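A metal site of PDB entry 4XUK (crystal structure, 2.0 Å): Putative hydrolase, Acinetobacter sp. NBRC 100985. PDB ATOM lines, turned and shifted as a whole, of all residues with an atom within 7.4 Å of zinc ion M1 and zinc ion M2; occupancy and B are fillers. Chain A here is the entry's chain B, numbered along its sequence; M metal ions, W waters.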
ATOM      1  N   SER A  57      16.837 -14.179  23.239  1.00  0.00           N
ATOM      2  CA  SER A  57      17.208 -15.396  23.964  1.00  0.00           C
ATOM      3  C   SER A  57      18.230 -15.047  25.051  1.00  0.00           C
ATOM      4  O   SER A  57      18.922 -14.026  24.952  1.00  0.00           O
ATOM      5  CB  SER A  57      17.776 -16.471  23.034  1.00  0.00           C
ATOM      6  OG  SER A  57      16.808 -16.953  22.121  1.00  0.00           O
ATOM      7  N   ILE A  58      18.266 -15.875  26.091  1.00  0.00           N
ATOM      8  CA  ILE A  58      19.357 -15.881  27.044  1.00  0.00           C
ATOM      9  C   ILE A  58      19.910 -17.306  27.070  1.00  0.00           C
ATOM     10  O   ILE A  58      19.213 -18.251  27.467  1.00  0.00           O
ATOM     11  CB  ILE A  58      18.912 -15.485  28.484  1.00  0.00           C
ATOM     12  CG1 ILE A  58      18.343 -14.072  28.538  1.00  0.00           C
ATOM     13  CG2 ILE A  58      20.086 -15.570  29.460  1.00  0.00           C
ATOM     14  CD1 ILE A  58      16.881 -13.967  28.136  1.00  0.00           C
ATOM     15  N   ASP A  73      29.329 -18.813  30.879  1.00  0.00           N
ATOM     16  CA  ASP A  73      28.115 -18.203  31.433  1.00  0.00           C
ATOM     17  C   ASP A  73      27.123 -19.251  31.952  1.00  0.00           C
ATOM     18  O   ASP A  73      27.286 -20.450  31.693  1.00  0.00           O
ATOM     19  CB  ASP A  73      27.463 -17.201  30.466  1.00  0.00           C
ATOM     20  CG  ASP A  73      28.367 -16.005  30.172  1.00  0.00           C
ATOM     21  OD1 ASP A  73      29.337 -15.778  30.932  1.00  0.00           O
ATOM     22  OD2 ASP A  73      28.111 -15.293  29.170  1.00  0.00           O
ATOM     23  N   PHE A  80      16.255 -12.634  37.997  1.00  0.00           N
ATOM     24  CA  PHE A  80      15.375 -11.760  37.208  1.00  0.00           C
ATOM     25  C   PHE A  80      13.942 -12.223  37.123  1.00  0.00           C
ATOM     26  O   PHE A  80      13.181 -11.655  36.398  1.00  0.00           O
ATOM     27  CB  PHE A  80      15.878 -11.517  35.773  1.00  0.00           C
ATOM     28  CG  PHE A  80      17.068 -10.623  35.676  1.00  0.00           C
ATOM     29  CD1 PHE A  80      17.094  -9.414  36.334  1.00  0.00           C
ATOM     30  CD2 PHE A  80      18.147 -10.983  34.947  1.00  0.00           C
ATOM     31  CE1 PHE A  80      18.197  -8.588  36.258  1.00  0.00           C
ATOM     32  CE2 PHE A  80      19.230 -10.171  34.858  1.00  0.00           C
ATOM     33  CZ  PHE A  80      19.260  -8.970  35.517  1.00  0.00           C
ATOM     34  N   THR A 107      31.772 -14.267  30.871  1.00  0.00           N
ATOM     35  CA  THR A 107      32.069 -13.161  29.976  1.00  0.00           C
ATOM     36  C   THR A 107      31.980 -11.832  30.724  1.00  0.00           C
ATOM     37  O   THR A 107      32.761 -10.916  30.474  1.00  0.00           O
ATOM     38  CB  THR A 107      31.125 -13.149  28.752  1.00  0.00           C
ATOM     39  OG1 THR A 107      29.767 -13.145  29.197  1.00  0.00           O
ATOM     40  CG2 THR A 107      31.373 -14.381  27.889  1.00  0.00           C
ATOM     41  N   HIS A 108      31.025 -11.748  31.656  1.00  0.00           N
ATOM     42  CA  HIS A 108      30.840 -10.574  32.519  1.00  0.00           C
ATOM     43  C   HIS A 108      29.966 -10.944  33.711  1.00  0.00           C
ATOM     44  O   HIS A 108      29.425 -12.059  33.770  1.00  0.00           O
ATOM     45  CB  HIS A 108      30.243  -9.370  31.758  1.00  0.00           C
ATOM     46  CG  HIS A 108      28.960  -9.659  31.053  1.00  0.00           C
ATOM     47  ND1 HIS A 108      27.842  -8.859  31.182  1.00  0.00           N
ATOM     48  CD2 HIS A 108      28.616 -10.631  30.177  1.00  0.00           C
ATOM     49  CE1 HIS A 108      26.865  -9.341  30.427  1.00  0.00           C
ATOM     50  NE2 HIS A 108      27.315 -10.412  29.802  1.00  0.00           N
ATOM     51  N   LEU A 109      29.826 -10.010  34.660  1.00  0.00           N
ATOM     52  CA  LEU A 109      29.122 -10.315  35.908  1.00  0.00           C
ATOM     53  C   LEU A 109      27.668  -9.834  35.965  1.00  0.00           C
ATOM     54  O   LEU A 109      27.064  -9.806  37.037  1.00  0.00           O
ATOM     55  CB  LEU A 109      29.912  -9.805  37.121  1.00  0.00           C
ATOM     56  CG  LEU A 109      31.284 -10.452  37.315  1.00  0.00           C
ATOM     57  CD1 LEU A 109      32.012  -9.865  38.492  1.00  0.00           C
ATOM     58  CD2 LEU A 109      31.186 -11.968  37.458  1.00  0.00           C
ATOM     59  N   HIS A 110      27.090  -9.487  34.825  1.00  0.00           N
ATOM     60  CA  HIS A 110      25.648  -9.227  34.782  1.00  0.00           C
ATOM     61  C   HIS A 110      24.897 -10.462  35.315  1.00  0.00           C
ATOM     62  O   HIS A 110      25.361 -11.592  35.127  1.00  0.00           O
ATOM     63  CB  HIS A 110      25.198  -8.840  33.368  1.00  0.00           C
ATOM     64  CG  HIS A 110      25.283  -7.367  33.112  1.00  0.00           C
ATOM     65  ND1 HIS A 110      25.309  -6.817  31.850  1.00  0.00           N
ATOM     66  CD2 HIS A 110      25.358  -6.314  33.972  1.00  0.00           C
ATOM     67  CE1 HIS A 110      25.386  -5.504  31.943  1.00  0.00           C
ATOM     68  NE2 HIS A 110      25.415  -5.175  33.221  1.00  0.00           N
ATOM     69  N   PRO A 111      23.767 -10.248  36.012  1.00  0.00           N
ATOM     70  CA  PRO A 111      23.088 -11.360  36.682  1.00  0.00           C
ATOM     71  C   PRO A 111      22.695 -12.483  35.733  1.00  0.00           C
ATOM     72  O   PRO A 111      22.754 -13.656  36.124  1.00  0.00           O
ATOM     73  CB  PRO A 111      21.842 -10.704  37.285  1.00  0.00           C
ATOM     74  CG  PRO A 111      22.271  -9.272  37.543  1.00  0.00           C
ATOM     75  CD  PRO A 111      23.178  -8.941  36.353  1.00  0.00           C
ATOM     76  N   ASP A 112      22.324 -12.147  34.492  1.00  0.00           N
ATOM     77  CA  ASP A 112      21.887 -13.178  33.553  1.00  0.00           C
ATOM     78  C   ASP A 112      23.038 -14.016  33.020  1.00  0.00           C
ATOM     79  O   ASP A 112      22.846 -14.870  32.150  1.00  0.00           O
ATOM     80  CB  ASP A 112      21.023 -12.585  32.426  1.00  0.00           C
ATOM     81  CG  ASP A 112      21.753 -11.518  31.621  1.00  0.00           C
ATOM     82  OD1 ASP A 112      22.372 -10.630  32.232  1.00  0.00           O
ATOM     83  OD2 ASP A 112      21.657 -11.559  30.377  1.00  0.00           O
ATOM     84  N   HIS A 113      24.226 -13.774  33.566  1.00  0.00           N
ATOM     85  CA  HIS A 113      25.416 -14.545  33.229  1.00  0.00           C
ATOM     86  C   HIS A 113      26.069 -15.244  34.442  1.00  0.00           C
ATOM     87  O   HIS A 113      26.599 -16.355  34.309  1.00  0.00           O
ATOM     88  CB  HIS A 113      26.385 -13.616  32.480  1.00  0.00           C
ATOM     89  CG  HIS A 113      25.814 -13.060  31.220  1.00  0.00           C
ATOM     90  ND1 HIS A 113      26.054 -13.616  29.981  1.00  0.00           N
ATOM     91  CD2 HIS A 113      24.944 -12.036  31.011  1.00  0.00           C
ATOM     92  CE1 HIS A 113      25.373 -12.956  29.064  1.00  0.00           C
ATOM     93  NE2 HIS A 113      24.707 -11.983  29.659  1.00  0.00           N
ATOM     94  N   GLU A 136      36.708  -6.831  35.306  1.00  0.00           N
ATOM     95  CA  GLU A 136      35.283  -7.029  35.609  1.00  0.00           C
ATOM     96  C   GLU A 136      35.034  -7.136  37.110  1.00  0.00           C
ATOM     97  O   GLU A 136      34.136  -6.460  37.630  1.00  0.00           O
ATOM     98  CB  GLU A 136      34.726  -8.252  34.872  1.00  0.00           C
ATOM     99  CG  GLU A 136      33.221  -8.462  35.048  1.00  0.00           C
ATOM    100  CD  GLU A 136      32.359  -7.500  34.236  1.00  0.00           C
ATOM    101  OE1 GLU A 136      32.930  -6.687  33.476  1.00  0.00           O
ATOM    102  OE2 GLU A 136      31.110  -7.565  34.351  1.00  0.00           O
ATOM    103  N   HIS A 197      30.327  -2.956  27.084  1.00  0.00           N
ATOM    104  CA  HIS A 197      29.049  -3.376  27.648  1.00  0.00           C
ATOM    105  C   HIS A 197      29.173  -3.380  29.167  1.00  0.00           C
ATOM    106  O   HIS A 197      28.288  -2.871  29.866  1.00  0.00           O
ATOM    107  CB  HIS A 197      28.674  -4.773  27.131  1.00  0.00           C
ATOM    108  CG  HIS A 197      27.455  -5.346  27.779  1.00  0.00           C
ATOM    109  ND1 HIS A 197      26.183  -4.865  27.559  1.00  0.00           N
ATOM    110  CD2 HIS A 197      27.315  -6.393  28.640  1.00  0.00           C
ATOM    111  CE1 HIS A 197      25.318  -5.571  28.260  1.00  0.00           C
ATOM    112  NE2 HIS A 197      25.980  -6.510  28.919  1.00  0.00           N
ATOM    113  N   THR A 198      30.256  -3.957  29.674  1.00  0.00           N
ATOM    114  CA  THR A 198      30.713  -3.726  31.045  1.00  0.00           C
ATOM    115  C   THR A 198      32.199  -3.425  30.957  1.00  0.00           C
ATOM    116  O   THR A 198      32.831  -3.740  29.952  1.00  0.00           O
ATOM    117  CB  THR A 198      30.484  -4.948  32.004  1.00  0.00           C
ATOM    118  OG1 THR A 198      31.253  -6.077  31.557  1.00  0.00           O
ATOM    119  CG2 THR A 198      28.989  -5.332  32.112  1.00  0.00           C
ATOM    120  N   HIS A 201      34.318  -6.661  30.360  1.00  0.00           N
ATOM    121  CA  HIS A 201      33.713  -7.684  29.495  1.00  0.00           C
ATOM    122  C   HIS A 201      34.738  -8.346  28.582  1.00  0.00           C
ATOM    123  O   HIS A 201      35.442  -7.655  27.823  1.00  0.00           O
ATOM    124  CB  HIS A 201      32.598  -7.072  28.643  1.00  0.00           C
ATOM    125  CG  HIS A 201      31.786  -8.082  27.887  1.00  0.00           C
ATOM    126  ND1 HIS A 201      32.267  -8.732  26.778  1.00  0.00           N
ATOM    127  CD2 HIS A 201      30.538  -8.549  28.090  1.00  0.00           C
ATOM    128  CE1 HIS A 201      31.347  -9.572  26.330  1.00  0.00           C
ATOM    129  NE2 HIS A 201      30.285  -9.483  27.115  1.00  0.00           N
ATOM    130  N   GLY A 217      29.943 -13.415  24.237  1.00  0.00           N
ATOM    131  CA  GLY A 217      29.295 -12.721  25.329  1.00  0.00           C
ATOM    132  C   GLY A 217      28.339 -11.662  24.827  1.00  0.00           C
ATOM    133  O   GLY A 217      27.695 -11.833  23.782  1.00  0.00           O
ATOM    134  N   ASP A 218      28.253 -10.551  25.560  1.00  0.00           N
ATOM    135  CA  ASP A 218      27.251  -9.530  25.263  1.00  0.00           C
ATOM    136  C   ASP A 218      27.722  -8.373  24.375  1.00  0.00           C
ATOM    137  O   ASP A 218      27.371  -7.219  24.629  1.00  0.00           O
ATOM    138  CB  ASP A 218      26.682  -8.975  26.568  1.00  0.00           C
ATOM    139  CG  ASP A 218      25.607  -9.866  27.152  1.00  0.00           C
ATOM    140  OD1 ASP A 218      25.562 -11.083  26.833  1.00  0.00           O
ATOM    141  OD2 ASP A 218      24.798  -9.331  27.914  1.00  0.00           O
ATOM    142  N   VAL A 220      26.569  -8.051  21.602  1.00  0.00           N
ATOM    143  CA  VAL A 220      25.390  -7.874  20.764  1.00  0.00           C
ATOM    144  C   VAL A 220      24.167  -8.456  21.456  1.00  0.00           C
ATOM    145  O   VAL A 220      24.269  -9.452  22.207  1.00  0.00           O
ATOM    146  CB  VAL A 220      25.609  -8.496  19.345  1.00  0.00           C
ATOM    147  CG1 VAL A 220      25.475 -10.009  19.380  1.00  0.00           C
ATOM    148  CG2 VAL A 220      24.671  -7.864  18.308  1.00  0.00           C
ATOM    149  N   HIS A 221      23.002  -7.848  21.230  1.00  0.00           N
ATOM    150  CA  HIS A 221      21.766  -8.284  21.861  1.00  0.00           C
ATOM    151  C   HIS A 221      20.639  -8.609  20.883  1.00  0.00           C
ATOM    152  O   HIS A 221      19.482  -8.761  21.301  1.00  0.00           O
ATOM    153  CB  HIS A 221      21.261  -7.215  22.832  1.00  0.00           C
ATOM    154  CG  HIS A 221      22.044  -7.140  24.089  1.00  0.00           C
ATOM    155  ND1 HIS A 221      23.307  -6.590  24.147  1.00  0.00           N
ATOM    156  CD2 HIS A 221      21.762  -7.556  25.351  1.00  0.00           C
ATOM    157  CE1 HIS A 221      23.774  -6.668  25.375  1.00  0.00           C
ATOM    158  NE2 HIS A 221      22.846  -7.242  26.132  1.00  0.00           N
ATOM    159  N   TYR A 236      21.373  -1.344  27.811  1.00  0.00           N
ATOM    160  CA  TYR A 236      22.073  -2.180  28.794  1.00  0.00           C
ATOM    161  C   TYR A 236      23.594  -1.955  28.882  1.00  0.00           C
ATOM    162  O   TYR A 236      24.207  -2.323  29.874  1.00  0.00           O
ATOM    163  CB  TYR A 236      21.873  -3.675  28.494  1.00  0.00           C
ATOM    164  CG  TYR A 236      20.456  -4.205  28.347  1.00  0.00           C
ATOM    165  CD1 TYR A 236      19.533  -4.105  29.373  1.00  0.00           C
ATOM    166  CD2 TYR A 236      20.070  -4.876  27.194  1.00  0.00           C
ATOM    167  CE1 TYR A 236      18.255  -4.601  29.244  1.00  0.00           C
ATOM    168  CE2 TYR A 236      18.799  -5.395  27.048  1.00  0.00           C
ATOM    169  CZ  TYR A 236      17.901  -5.244  28.089  1.00  0.00           C
ATOM    170  OH  TYR A 236      16.623  -5.750  27.983  1.00  0.00           O
ATOM    171  N   ASP A 237      24.203  -1.419  27.821  1.00  0.00           N
ATOM    172  CA  ASP A 237      25.649  -1.154  27.811  1.00  0.00           C
ATOM    173  C   ASP A 237      25.985  -0.087  28.856  1.00  0.00           C
ATOM    174  O   ASP A 237      25.325   0.955  28.905  1.00  0.00           O
ATOM    175  CB  ASP A 237      26.109  -0.630  26.438  1.00  0.00           C
ATOM    176  CG  ASP A 237      26.004  -1.672  25.311  1.00  0.00           C
ATOM    177  OD1 ASP A 237      26.264  -2.878  25.544  1.00  0.00           O
ATOM    178  OD2 ASP A 237      25.695  -1.257  24.176  1.00  0.00           O
ATOM    179  N   PRO A 264      25.288 -15.477  23.898  1.00  0.00           N
ATOM    180  CA  PRO A 264      24.219 -15.632  24.894  1.00  0.00           C
ATOM    181  C   PRO A 264      22.923 -14.915  24.534  1.00  0.00           C
ATOM    182  O   PRO A 264      21.895 -15.265  25.116  1.00  0.00           O
ATOM    183  CB  PRO A 264      24.830 -15.029  26.174  1.00  0.00           C
ATOM    184  CG  PRO A 264      25.923 -14.137  25.721  1.00  0.00           C
ATOM    185  CD  PRO A 264      26.448 -14.737  24.425  1.00  0.00           C
ATOM    186  N   HIS A 265      22.943 -13.940  23.618  1.00  0.00           N
ATOM    187  CA  HIS A 265      21.719 -13.203  23.302  1.00  0.00           C
ATOM    188  C   HIS A 265      21.370 -13.192  21.815  1.00  0.00           C
ATOM    189  O   HIS A 265      20.633 -12.321  21.332  1.00  0.00           O
ATOM    190  CB  HIS A 265      21.782 -11.767  23.851  1.00  0.00           C
ATOM    191  CG  HIS A 265      21.771 -11.689  25.337  1.00  0.00           C
ATOM    192  ND1 HIS A 265      20.841 -12.365  26.107  1.00  0.00           N
ATOM    193  CD2 HIS A 265      22.562 -11.021  26.213  1.00  0.00           C
ATOM    194  CE1 HIS A 265      21.065 -12.101  27.381  1.00  0.00           C
ATOM    195  NE2 HIS A 265      22.100 -11.295  27.469  1.00  0.00           N
HETATM  196 ZN    ZN M   1      23.429 -10.598  29.150  1.00  0.00          ZN
HETATM  197 ZN    ZN M   2      25.286  -8.115  30.074  1.00  0.00          ZN
HETATM  198  O   HOH W   1      22.580  -7.469  29.226  1.00  0.00           O
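Merely in contact with zinc ion M2: His 108 (2.0 Å). Of the 23 residues printed, 5 come within 4 Å of zinc ion M2. Along chain A the residues within 4 Å of zinc ion M2 span positions 108 to 218. The nearest printed residue that does not touch zinc ion M2 is Asp 112 (4.4 Å).
Zinc ion M2 is bound by NE2 of His 197 (2.1 Å), ND1 of His 110 (2.2 Å) and OD2 of Asp 218 (2.5 Å). Zinc ion M2 has three donor atoms within binding distance.
Zinc ion M1 is bound by NE2 of His 113, 2.0 Å away. Zinc ion M1 is bound by OD2 of Asp 218 (2.2 Å). A ring nitrogen (NE2) of His 265 binds zinc ion M1 (2.3 Å). OD2 of Asp 112 binds zinc ion M1, 2.4 Å away. Zinc ion M1 has four donor atoms within binding distance.
A ring nitrogen (ND1) of His 113 sits close to a ring nitrogen (NE2) of His 108 (3.4 Å). ND1 of His 113 is in hydrogen-bond range of OD2 of Asp 73. ND1 of His 108 sits close to ND1 of His 110, 3.3 Å away. A ring nitrogen (NE2) of His 108 sits close to the side-chain carboxylate (OD2) of Asp 218 (3.3 Å). A ring nitrogen (ND1) of His 197 is in hydrogen-bond range of the side-chain carboxylate of Asp 237 (2.8 Å). The side-chain carboxylate (OD2) of Asp 218 lies close to a ring nitrogen (NE2) of His 221. N of Asp 218 sits at hydrogen-bond distance from NE2 of His 201, at 2.8 Å. The backbone carbonyl oxygen (O) of Ser 57 sits at hydrogen-bond distance from a ring nitrogen (ND1) of His 265, 2.8 Å away.
His 108 touches zinc ion M1 (CE1 to ZN, 3.9 Å). Of the 23 residues printed, 5 come within 4 Å of zinc ion M1. The nearest printed residue that does not touch zinc ion M1 is His 221 (4.6 Å).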
